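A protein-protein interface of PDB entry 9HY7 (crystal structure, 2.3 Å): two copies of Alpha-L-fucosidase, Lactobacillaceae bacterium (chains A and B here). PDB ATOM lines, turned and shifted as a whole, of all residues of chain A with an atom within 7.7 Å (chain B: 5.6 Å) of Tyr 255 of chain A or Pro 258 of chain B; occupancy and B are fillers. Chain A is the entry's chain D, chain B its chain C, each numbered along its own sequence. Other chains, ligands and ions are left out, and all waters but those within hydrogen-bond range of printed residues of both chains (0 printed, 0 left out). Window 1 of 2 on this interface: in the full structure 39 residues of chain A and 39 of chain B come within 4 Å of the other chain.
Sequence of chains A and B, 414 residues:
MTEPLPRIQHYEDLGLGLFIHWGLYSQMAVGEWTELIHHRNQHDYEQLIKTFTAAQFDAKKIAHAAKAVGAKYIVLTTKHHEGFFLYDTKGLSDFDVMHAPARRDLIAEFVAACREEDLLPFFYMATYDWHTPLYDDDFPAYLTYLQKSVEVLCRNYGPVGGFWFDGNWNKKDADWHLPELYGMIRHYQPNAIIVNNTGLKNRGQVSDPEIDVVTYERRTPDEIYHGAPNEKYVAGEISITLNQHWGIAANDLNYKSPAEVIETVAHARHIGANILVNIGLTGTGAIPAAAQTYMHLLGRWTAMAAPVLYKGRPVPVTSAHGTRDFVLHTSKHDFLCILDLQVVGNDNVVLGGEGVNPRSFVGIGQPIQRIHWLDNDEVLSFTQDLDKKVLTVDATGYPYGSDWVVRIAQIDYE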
ATOM      1  N   THR A 241       8.460  -6.730   5.720  1.00  0.00           N
ATOM      2  CA  THR A 241       7.044  -7.056   5.659  1.00  0.00           C
ATOM      3  C   THR A 241       6.822  -8.027   4.489  1.00  0.00           C
ATOM      4  O   THR A 241       7.659  -8.116   3.591  1.00  0.00           O
ATOM      5  CB  THR A 241       6.231  -5.754   5.545  1.00  0.00           C
ATOM      6  OG1 THR A 241       4.874  -6.116   5.842  1.00  0.00           O
ATOM      7  CG2 THR A 241       6.439  -5.003   4.226  1.00  0.00           C
ATOM      8  N   LEU A 242       5.701  -8.751   4.510  1.00  0.00           N
ATOM      9  CA  LEU A 242       5.523  -9.879   3.600  1.00  0.00           C
ATOM     10  C   LEU A 242       5.176  -9.404   2.184  1.00  0.00           C
ATOM     11  O   LEU A 242       5.615 -10.020   1.218  1.00  0.00           O
ATOM     12  CB  LEU A 242       4.518 -10.904   4.142  1.00  0.00           C
ATOM     13  CG  LEU A 242       4.873 -11.524   5.504  1.00  0.00           C
ATOM     14  CD1 LEU A 242       3.758 -12.439   5.980  1.00  0.00           C
ATOM     15  CD2 LEU A 242       6.222 -12.261   5.491  1.00  0.00           C
ATOM     16  N   ASN A 243       4.391  -8.321   2.054  1.00  0.00           N
ATOM     17  CA  ASN A 243       4.127  -7.693   0.757  1.00  0.00           C
ATOM     18  C   ASN A 243       4.699  -6.270   0.769  1.00  0.00           C
ATOM     19  O   ASN A 243       5.785  -6.062   1.292  1.00  0.00           O
ATOM     20  CB  ASN A 243       2.666  -7.844   0.325  1.00  0.00           C
ATOM     21  CG  ASN A 243       1.679  -7.294   1.334  1.00  0.00           C
ATOM     22  OD1 ASN A 243       2.064  -6.551   2.247  1.00  0.00           O
ATOM     23  ND2 ASN A 243       0.401  -7.604   1.167  1.00  0.00           N
ATOM     24  N   GLN A 244       3.976  -5.289   0.220  1.00  0.00           N
ATOM     25  CA  GLN A 244       4.508  -3.939   0.154  1.00  0.00           C
ATOM     26  C   GLN A 244       4.018  -3.071   1.330  1.00  0.00           C
ATOM     27  O   GLN A 244       4.517  -1.960   1.536  1.00  0.00           O
ATOM     28  CB  GLN A 244       4.129  -3.298  -1.180  1.00  0.00           C
ATOM     29  CG  GLN A 244       4.856  -3.887  -2.381  1.00  0.00           C
ATOM     30  CD  GLN A 244       6.346  -3.594  -2.347  1.00  0.00           C
ATOM     31  OE1 GLN A 244       6.780  -2.426  -2.382  1.00  0.00           O
ATOM     32  NE2 GLN A 244       7.132  -4.654  -2.261  1.00  0.00           N
ATOM     33  N   ILE A 248      -2.662  -4.534   6.906  1.00  0.00           N
ATOM     34  CA  ILE A 248      -3.208  -5.439   5.919  1.00  0.00           C
ATOM     35  C   ILE A 248      -3.623  -4.642   4.668  1.00  0.00           C
ATOM     36  O   ILE A 248      -4.089  -3.491   4.737  1.00  0.00           O
ATOM     37  CB  ILE A 248      -4.387  -6.233   6.521  1.00  0.00           C
ATOM     38  CG1 ILE A 248      -4.858  -7.382   5.579  1.00  0.00           C
ATOM     39  CG2 ILE A 248      -5.557  -5.300   6.924  1.00  0.00           C
ATOM     40  CD1 ILE A 248      -5.794  -8.379   6.253  1.00  0.00           C
ATOM     41  N   ALA A 249      -3.435  -5.265   3.503  1.00  0.00           N
ATOM     42  CA  ALA A 249      -3.735  -4.655   2.218  1.00  0.00           C
ATOM     43  C   ALA A 249      -4.225  -5.757   1.284  1.00  0.00           C
ATOM     44  O   ALA A 249      -3.422  -6.488   0.705  1.00  0.00           O
ATOM     45  CB  ALA A 249      -2.490  -3.953   1.684  1.00  0.00           C
ATOM     46  N   ALA A 250      -5.556  -5.875   1.169  1.00  0.00           N
ATOM     47  CA  ALA A 250      -6.205  -7.035   0.567  1.00  0.00           C
ATOM     48  C   ALA A 250      -5.800  -7.218  -0.896  1.00  0.00           C
ATOM     49  O   ALA A 250      -5.687  -8.355  -1.340  1.00  0.00           O
ATOM     50  CB  ALA A 250      -7.730  -6.937   0.688  1.00  0.00           C
ATOM     51  N   ASN A 251      -5.620  -6.121  -1.648  1.00  0.00           N
ATOM     52  CA  ASN A 251      -5.283  -6.228  -3.053  1.00  0.00           C
ATOM     53  C   ASN A 251      -3.808  -5.949  -3.316  1.00  0.00           C
ATOM     54  O   ASN A 251      -3.434  -5.553  -4.428  1.00  0.00           O
ATOM     55  CB  ASN A 251      -6.181  -5.329  -3.903  1.00  0.00           C
ATOM     56  CG  ASN A 251      -7.583  -5.926  -3.981  1.00  0.00           C
ATOM     57  OD1 ASN A 251      -7.775  -7.156  -4.059  1.00  0.00           O
ATOM     58  ND2 ASN A 251      -8.594  -5.086  -3.869  1.00  0.00           N
ATOM     59  N   ASP A 252      -2.966  -6.131  -2.295  1.00  0.00           N
ATOM     60  CA  ASP A 252      -1.526  -6.145  -2.536  1.00  0.00           C
ATOM     61  C   ASP A 252      -1.121  -7.616  -2.699  1.00  0.00           C
ATOM     62  O   ASP A 252      -1.027  -8.344  -1.706  1.00  0.00           O
ATOM     63  CB  ASP A 252      -0.774  -5.454  -1.404  1.00  0.00           C
ATOM     64  CG  ASP A 252       0.745  -5.530  -1.459  1.00  0.00           C
ATOM     65  OD1 ASP A 252       1.265  -6.160  -2.403  1.00  0.00           O
ATOM     66  OD2 ASP A 252       1.417  -4.943  -0.560  1.00  0.00           O
ATOM     67  N   LEU A 253      -0.880  -8.041  -3.945  1.00  0.00           N
ATOM     68  CA  LEU A 253      -0.555  -9.436  -4.260  1.00  0.00           C
ATOM     69  C   LEU A 253       0.959  -9.587  -4.362  1.00  0.00           C
ATOM     70  O   LEU A 253       1.455 -10.674  -4.656  1.00  0.00           O
ATOM     71  CB  LEU A 253      -1.214  -9.814  -5.590  1.00  0.00           C
ATOM     72  CG  LEU A 253      -2.705  -9.444  -5.737  1.00  0.00           C
ATOM     73  CD1 LEU A 253      -3.339  -9.904  -7.045  1.00  0.00           C
ATOM     74  CD2 LEU A 253      -3.572  -9.875  -4.529  1.00  0.00           C
ATOM     75  N   ASN A 254       1.708  -8.493  -4.147  1.00  0.00           N
ATOM     76  CA  ASN A 254       3.144  -8.505  -4.386  1.00  0.00           C
ATOM     77  C   ASN A 254       3.887  -9.055  -3.159  1.00  0.00           C
ATOM     78  O   ASN A 254       4.681  -8.346  -2.534  1.00  0.00           O
ATOM     79  CB  ASN A 254       3.596  -7.112  -4.819  1.00  0.00           C
ATOM     80  CG  ASN A 254       5.027  -7.080  -5.281  1.00  0.00           C
ATOM     81  OD1 ASN A 254       5.621  -8.132  -5.533  1.00  0.00           O
ATOM     82  ND2 ASN A 254       5.592  -5.903  -5.476  1.00  0.00           N
ATOM     83  N   TYR A 255       3.645 -10.327  -2.826  1.00  0.00           N
ATOM     84  CA  TYR A 255       4.298 -10.996  -1.705  1.00  0.00           C
ATOM     85  C   TYR A 255       5.676 -11.491  -2.118  1.00  0.00           C
ATOM     86  O   TYR A 255       5.875 -11.950  -3.259  1.00  0.00           O
ATOM     87  CB  TYR A 255       3.445 -12.192  -1.278  1.00  0.00           C
ATOM     88  CG  TYR A 255       2.297 -11.848  -0.336  1.00  0.00           C
ATOM     89  CD1 TYR A 255       1.142 -11.257  -0.819  1.00  0.00           C
ATOM     90  CD2 TYR A 255       2.393 -12.088   1.035  1.00  0.00           C
ATOM     91  CE1 TYR A 255       0.083 -10.948   0.026  1.00  0.00           C
ATOM     92  CE2 TYR A 255       1.361 -11.769   1.905  1.00  0.00           C
ATOM     93  CZ  TYR A 255       0.207 -11.191   1.389  1.00  0.00           C
ATOM     94  OH  TYR A 255      -0.845 -10.865   2.193  1.00  0.00           O
ATOM     95  N   LYS A 256       6.626 -11.387  -1.177  1.00  0.00           N
ATOM     96  CA  LYS A 256       7.965 -11.932  -1.342  1.00  0.00           C
ATOM     97  C   LYS A 256       7.898 -13.455  -1.265  1.00  0.00           C
ATOM     98  O   LYS A 256       6.930 -14.011  -0.725  1.00  0.00           O
ATOM     99  CB  LYS A 256       8.828 -11.375  -0.204  1.00  0.00           C
ATOM    100  CG  LYS A 256       8.984  -9.862  -0.208  1.00  0.00           C
ATOM    101  CD  LYS A 256       9.814  -9.330   0.979  1.00  0.00           C
ATOM    102  CE  LYS A 256       9.761  -7.792   1.113  1.00  0.00           C
ATOM    103  NZ  LYS A 256       8.401  -7.245   0.968  1.00  0.00           N
ATOM    104  N   SER A 257       8.905 -14.141  -1.821  1.00  0.00           N
ATOM    105  CA  SER A 257       8.932 -15.583  -1.620  1.00  0.00           C
ATOM    106  C   SER A 257       9.249 -15.911  -0.158  1.00  0.00           C
ATOM    107  O   SER A 257       9.986 -15.173   0.506  1.00  0.00           O
ATOM    108  CB  SER A 257       9.892 -16.284  -2.542  1.00  0.00           C
ATOM    109  OG  SER A 257      11.216 -15.908  -2.214  1.00  0.00           O
ATOM    110  N   PRO A 258       8.676 -17.015   0.379  1.00  0.00           N
ATOM    111  CA  PRO A 258       9.145 -17.567   1.659  1.00  0.00           C
ATOM    112  C   PRO A 258      10.662 -17.744   1.708  1.00  0.00           C
ATOM    113  O   PRO A 258      11.287 -17.481   2.734  1.00  0.00           O
ATOM    114  CB  PRO A 258       8.319 -18.833   1.836  1.00  0.00           C
ATOM    115  CG  PRO A 258       7.064 -18.571   0.986  1.00  0.00           C
ATOM    116  CD  PRO A 258       7.498 -17.711  -0.181  1.00  0.00           C
ATOM    117  N   GLU A 260      12.905 -15.862   0.199  1.00  0.00           N
ATOM    118  CA  GLU A 260      13.531 -14.574   0.454  1.00  0.00           C
ATOM    119  C   GLU A 260      13.412 -14.195   1.947  1.00  0.00           C
ATOM    120  O   GLU A 260      14.326 -13.598   2.524  1.00  0.00           O
ATOM    121  CB  GLU A 260      12.996 -13.491  -0.477  1.00  0.00           C
ATOM    122  CG  GLU A 260      13.551 -12.096  -0.150  1.00  0.00           C
ATOM    123  CD  GLU A 260      13.006 -10.954  -1.019  1.00  0.00           C
ATOM    124  OE1 GLU A 260      12.280 -11.209  -2.017  1.00  0.00           O
ATOM    125  OE2 GLU A 260      13.239  -9.781  -0.669  1.00  0.00           O
ATOM    126  N   VAL A 261      12.291 -14.544   2.580  1.00  0.00           N
ATOM    127  CA  VAL A 261      12.124 -14.260   3.995  1.00  0.00           C
ATOM    128  C   VAL A 261      13.194 -15.009   4.819  1.00  0.00           C
ATOM    129  O   VAL A 261      13.860 -14.418   5.680  1.00  0.00           O
ATOM    130  CB  VAL A 261      10.679 -14.560   4.461  1.00  0.00           C
ATOM    131  CG1 VAL A 261      10.534 -14.436   5.986  1.00  0.00           C
ATOM    132  CG2 VAL A 261       9.672 -13.671   3.722  1.00  0.00           C
ATOM    133  N   GLY A 280       0.246  -7.908   9.296  1.00  0.00           N
ATOM    134  CA  GLY A 280      -0.839  -6.963   9.545  1.00  0.00           C
ATOM    135  C   GLY A 280      -2.131  -7.712   9.869  1.00  0.00           C
ATOM    136  O   GLY A 280      -2.558  -8.565   9.080  1.00  0.00           O
ATOM    137  N   PRO A 288      -4.203 -12.997   9.414  1.00  0.00           N
ATOM    138  CA  PRO A 288      -4.666 -13.507   8.124  1.00  0.00           C
ATOM    139  C   PRO A 288      -4.021 -14.832   7.727  1.00  0.00           C
ATOM    140  O   PRO A 288      -2.900 -15.159   8.150  1.00  0.00           O
ATOM    141  CB  PRO A 288      -4.445 -12.349   7.162  1.00  0.00           C
ATOM    142  CG  PRO A 288      -3.323 -11.563   7.830  1.00  0.00           C
ATOM    143  CD  PRO A 288      -3.378 -11.783   9.316  1.00  0.00           C
ATOM    144  N   ALA A 289      -4.740 -15.582   6.883  1.00  0.00           N
ATOM    145  CA  ALA A 289      -4.335 -16.915   6.426  1.00  0.00           C
ATOM    146  C   ALA A 289      -2.993 -16.847   5.693  1.00  0.00           C
ATOM    147  O   ALA A 289      -2.132 -17.706   5.890  1.00  0.00           O
ATOM    148  CB  ALA A 289      -5.444 -17.552   5.573  1.00  0.00           C
ATOM    149  N   ALA A 290      -2.794 -15.819   4.861  1.00  0.00           N
ATOM    150  CA  ALA A 290      -1.545 -15.696   4.117  1.00  0.00           C
ATOM    151  C   ALA A 290      -0.352 -15.577   5.082  1.00  0.00           C
ATOM    152  O   ALA A 290       0.687 -16.215   4.864  1.00  0.00           O
ATOM    153  CB  ALA A 290      -1.618 -14.560   3.121  1.00  0.00           C
ATOM    154  N   ALA A 291      -0.485 -14.768   6.146  1.00  0.00           N
ATOM    155  CA  ALA A 291       0.606 -14.607   7.097  1.00  0.00           C
ATOM    156  C   ALA A 291       0.952 -15.942   7.770  1.00  0.00           C
ATOM    157  O   ALA A 291       2.128 -16.239   8.003  1.00  0.00           O
ATOM    158  CB  ALA A 291       0.286 -13.522   8.126  1.00  0.00           C
ATOM    159  N   TYR A 294       3.385 -18.083   5.765  1.00  0.00           N
ATOM    160  CA  TYR A 294       4.762 -17.638   5.910  1.00  0.00           C
ATOM    161  C   TYR A 294       5.332 -18.038   7.273  1.00  0.00           C
ATOM    162  O   TYR A 294       6.492 -18.443   7.374  1.00  0.00           O
ATOM    163  CB  TYR A 294       4.879 -16.133   5.677  1.00  0.00           C
ATOM    164  CG  TYR A 294       4.804 -15.831   4.188  1.00  0.00           C
ATOM    165  CD1 TYR A 294       3.599 -15.844   3.482  1.00  0.00           C
ATOM    166  CD2 TYR A 294       5.961 -15.540   3.493  1.00  0.00           C
ATOM    167  CE1 TYR A 294       3.563 -15.545   2.119  1.00  0.00           C
ATOM    168  CE2 TYR A 294       5.948 -15.247   2.133  1.00  0.00           C
ATOM    169  CZ  TYR A 294       4.747 -15.261   1.441  1.00  0.00           C
ATOM    170  OH  TYR A 294       4.743 -15.015   0.097  1.00  0.00           O
ATOM    171  N   LYS B 256       8.119 -20.315  -4.428  1.00  0.00           N
ATOM    172  CA  LYS B 256       8.178 -19.147  -5.292  1.00  0.00           C
ATOM    173  C   LYS B 256       7.306 -18.040  -4.699  1.00  0.00           C
ATOM    174  O   LYS B 256       6.403 -18.307  -3.908  1.00  0.00           O
ATOM    175  CB  LYS B 256       7.640 -19.565  -6.666  1.00  0.00           C
ATOM    176  CG  LYS B 256       8.499 -20.671  -7.347  1.00  0.00           C
ATOM    177  CD  LYS B 256       7.946 -21.104  -8.706  1.00  0.00           C
ATOM    178  CE  LYS B 256       8.610 -22.326  -9.292  1.00  0.00           C
ATOM    179  NZ  LYS B 256       8.770 -23.418  -8.323  1.00  0.00           N
ATOM    180  N   SER B 257       7.582 -16.783  -5.068  1.00  0.00           N
ATOM    181  CA  SER B 257       6.698 -15.725  -4.617  1.00  0.00           C
ATOM    182  C   SER B 257       5.369 -15.835  -5.353  1.00  0.00           C
ATOM    183  O   SER B 257       5.324 -16.258  -6.520  1.00  0.00           O
ATOM    184  CB  SER B 257       7.295 -14.345  -4.796  1.00  0.00           C
ATOM    185  OG  SER B 257       7.451 -14.068  -6.174  1.00  0.00           O
ATOM    186  N   PRO B 258       4.253 -15.446  -4.681  1.00  0.00           N
ATOM    187  CA  PRO B 258       2.988 -15.206  -5.374  1.00  0.00           C
ATOM    188  C   PRO B 258       3.146 -14.331  -6.618  1.00  0.00           C
ATOM    189  O   PRO B 258       2.528 -14.593  -7.640  1.00  0.00           O
ATOM    190  CB  PRO B 258       2.077 -14.666  -4.268  1.00  0.00           C
ATOM    191  CG  PRO B 258       2.667 -15.303  -3.004  1.00  0.00           C
ATOM    192  CD  PRO B 258       4.146 -15.310  -3.216  1.00  0.00           C
ATOM    193  N   ALA B 259       4.008 -13.313  -6.539  1.00  0.00           N
ATOM    194  CA  ALA B 259       4.269 -12.407  -7.659  1.00  0.00           C
ATOM    195  C   ALA B 259       4.820 -13.190  -8.848  1.00  0.00           C
ATOM    196  O   ALA B 259       4.422 -12.936  -9.985  1.00  0.00           O
ATOM    197  CB  ALA B 259       5.243 -11.290  -7.268  1.00  0.00           C
ATOM    198  N   GLU B 260       5.772 -14.109  -8.596  1.00  0.00           N
ATOM    199  CA  GLU B 260       6.315 -14.893  -9.699  1.00  0.00           C
ATOM    200  C   GLU B 260       5.226 -15.785 -10.324  1.00  0.00           C
ATOM    201  O   GLU B 260       5.196 -16.009 -11.548  1.00  0.00           O
ATOM    202  CB  GLU B 260       7.561 -15.676  -9.273  1.00  0.00           C
ATOM    203  CG  GLU B 260       8.074 -16.599 -10.380  1.00  0.00           C
ATOM    204  CD  GLU B 260       9.265 -17.489 -10.016  1.00  0.00           C
ATOM    205  OE1 GLU B 260       9.872 -17.326  -8.927  1.00  0.00           O
ATOM    206  OE2 GLU B 260       9.590 -18.400 -10.811  1.00  0.00           O
ATOM    207  N   VAL B 261       4.322 -16.314  -9.496  1.00  0.00           N
ATOM    208  CA  VAL B 261       3.242 -17.148 -10.008  1.00  0.00           C
ATOM    209  C   VAL B 261       2.345 -16.340 -10.956  1.00  0.00           C
ATOM    210  O   VAL B 261       2.041 -16.787 -12.074  1.00  0.00           O
ATOM    211  CB  VAL B 261       2.477 -17.858  -8.870  1.00  0.00           C
ATOM    212  CG1 VAL B 261       1.288 -18.652  -9.423  1.00  0.00           C
ATOM    213  CG2 VAL B 261       3.410 -18.796  -8.085  1.00  0.00           C
ATOM    214  N   ILE B 262       1.974 -15.116 -10.527  1.00  0.00           N
ATOM    215  CA  ILE B 262       1.171 -14.223 -11.346  1.00  0.00           C
ATOM    216  C   ILE B 262       1.897 -13.933 -12.654  1.00  0.00           C
ATOM    217  O   ILE B 262       1.289 -14.018 -13.731  1.00  0.00           O
ATOM    218  CB  ILE B 262       0.777 -12.938 -10.575  1.00  0.00           C
ATOM    219  CG1 ILE B 262      -0.211 -13.271  -9.464  1.00  0.00           C
ATOM    220  CG2 ILE B 262       0.218 -11.873 -11.529  1.00  0.00           C
ATOM    221  CD1 ILE B 262      -0.443 -12.193  -8.426  1.00  0.00           C
ATOM    222  N   GLU B 263       3.189 -13.572 -12.580  1.00  0.00           N
ATOM    223  CA  GLU B 263       3.944 -13.259 -13.788  1.00  0.00           C
ATOM    224  C   GLU B 263       3.988 -14.461 -14.746  1.00  0.00           C
ATOM    225  O   GLU B 263       3.926 -14.270 -15.963  1.00  0.00           O
ATOM    226  CB  GLU B 263       5.365 -12.759 -13.513  1.00  0.00           C
ATOM    227  CG  GLU B 263       5.396 -11.357 -12.906  1.00  0.00           C
ATOM    228  CD  GLU B 263       6.767 -10.666 -12.815  1.00  0.00           C
ATOM    229  OE1 GLU B 263       7.776 -11.272 -13.253  1.00  0.00           O
ATOM    230  OE2 GLU B 263       6.842  -9.494 -12.357  1.00  0.00           O
ATOM    231  N   TYR B 294      -1.694 -19.414  -2.017  1.00  0.00           N
ATOM    232  CA  TYR B 294      -1.378 -19.120  -3.403  1.00  0.00           C
ATOM    233  C   TYR B 294      -2.634 -19.019  -4.255  1.00  0.00           C
ATOM    234  O   TYR B 294      -2.725 -18.130  -5.114  1.00  0.00           O
ATOM    235  CB  TYR B 294      -0.392 -20.162  -3.949  1.00  0.00           C
ATOM    236  CG  TYR B 294       1.006 -19.849  -3.438  1.00  0.00           C
ATOM    237  CD1 TYR B 294       1.408 -20.262  -2.171  1.00  0.00           C
ATOM    238  CD2 TYR B 294       1.919 -19.165  -4.219  1.00  0.00           C
ATOM    239  CE1 TYR B 294       2.687 -19.968  -1.692  1.00  0.00           C
ATOM    240  CE2 TYR B 294       3.192 -18.865  -3.756  1.00  0.00           C
ATOM    241  CZ  TYR B 294       3.568 -19.243  -2.476  1.00  0.00           C
ATOM    242  OH  TYR B 294       4.816 -18.945  -2.007  1.00  0.00           O
ATOM    243  N   LEU B 297      -4.394 -15.653  -3.573  1.00  0.00           N
ATOM    244  CA  LEU B 297      -3.692 -14.516  -4.161  1.00  0.00           C
ATOM    245  C   LEU B 297      -3.816 -14.517  -5.682  1.00  0.00           C
ATOM    246  O   LEU B 297      -4.218 -13.506  -6.274  1.00  0.00           O
ATOM    247  CB  LEU B 297      -2.241 -14.424  -3.685  1.00  0.00           C
ATOM    248  CG  LEU B 297      -2.084 -14.123  -2.176  1.00  0.00           C
ATOM    249  CD1 LEU B 297      -0.657 -14.395  -1.685  1.00  0.00           C
ATOM    250  CD2 LEU B 297      -2.524 -12.672  -1.843  1.00  0.00           C
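Of the printed residues of chain B, Tyr 255 of chain A touches Ser 257, Pro 258 and Leu 297.
Pro 258 of chain B touches just these residues of chain A: Tyr 255, Lys 256 and Tyr 294.
Of the printed residues of chain B, Ser 257 of chain A touches Lys 256 (3.8 Å) and Ser 257 (3.4 Å).
Of the printed residues of chain A, Leu 297 of chain B touches Leu 253 and Tyr 255.
Of the printed residues of chain A, Tyr 294 of chain B touches Pro 258.
Ala 250 of chain A touches none of the printed residues of chain B.
Thr 241 of chain A touches none of the printed residues of chain B.
The nearest printed residue of chain B that does not touch Tyr 255 of chain A is Ala 259 of chain B (4.01 Å).
The side-chain hydroxyl of Ser 257 of chain B sits at hydrogen-bond distance from the backbone NH of Glu 260 of chain B.
The backbone carbonyl oxygen (O) of Thr 241 of chain A lies within hydrogen-bond range of the side-chain amino group (NZ) of Lys 256 of chain A.
O of Leu 242 of chain A is in hydrogen-bond range of N of Lys 256 of chain A (2.9 Å).
O of Asn 243 of chain A lies within hydrogen-bond range of NZ of Lys 256 of chain A (2.9 Å).
The backbone carbonyl oxygen (O) of Lys 256 of chain A lies within hydrogen-bond range of the side-chain hydroxyl (OH) of Tyr 294 of chain A, 2.5 Å away.
OG of Ser 257 of chain A lies within hydrogen-bond range of N of Glu 260 of chain A, 2.9 Å away.
Hydrophobic or aromatic side chains of chain A that line the printed part of chain B: Leu 253, Tyr 255, Pro 258 and Tyr 294.
Printed residues of chain B that touch a printed residue of chain A: Lys 256, Ser 257, Pro 258, Ala 259, Ile 262, Tyr 294 and Leu 297.
Hydrophobic or aromatic side chains of chain B within 4 Å of the printed part of chain A: Pro 258, Ala 259, Ile 262, Tyr 294 and Leu 297.
Among the printed residues, 13 pairs touch across the chains.
Among the printed residues, no Asp or Glu carboxylate lies within 4 Å of a Lys or Arg side-chain nitrogen of the other chain.
Lys 256 of chain A touches Ser 257 of chain B, and with the chains exchanged Ser 257 of chain A touches Lys 256 of chain B.
Lys 256 of chain A touches Pro 258 of chain B, and with the chains exchanged Pro 258 of chain A touches Lys 256 of chain B.
Ser 257 of chain B touches its own counterpart, Ser 257 of chain A.
Pro 258 of chain A touches Tyr 294 of chain B, and with the chains exchanged Tyr 294 of chain A touches Pro 258 of chain B.
Of the 13 pairs that touch across the chains among the printed residues, 7 have their exchanged pair printed and touching as well.
Among the printed residues, pairs that only touch across the chains: Leu 253 of chain A with Ile 262 of chain B, Leu 253 of chain A with Leu 297 of chain B, Asn 254 of chain A with Ala 259 of chain B, Tyr 255 of chain A with Ser 257 of chain B, Tyr 255 of chain A with Pro 258 of chain B, Tyr 255 of chain A with Leu 297 of chain B, Lys 256 of chain A with Ser 257 of chain B, Lys 256 of chain A with Pro 258 of chain B, Ser 257 of chain A with Lys 256 of chain B, Ser 257 of chain A with Ser 257 of chain B, Pro 258 of chain A with Lys 256 of chain B, Pro 258 of chain A with Tyr 294 of chain B and Tyr 294 of chain A with Pro 258 of chain B.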
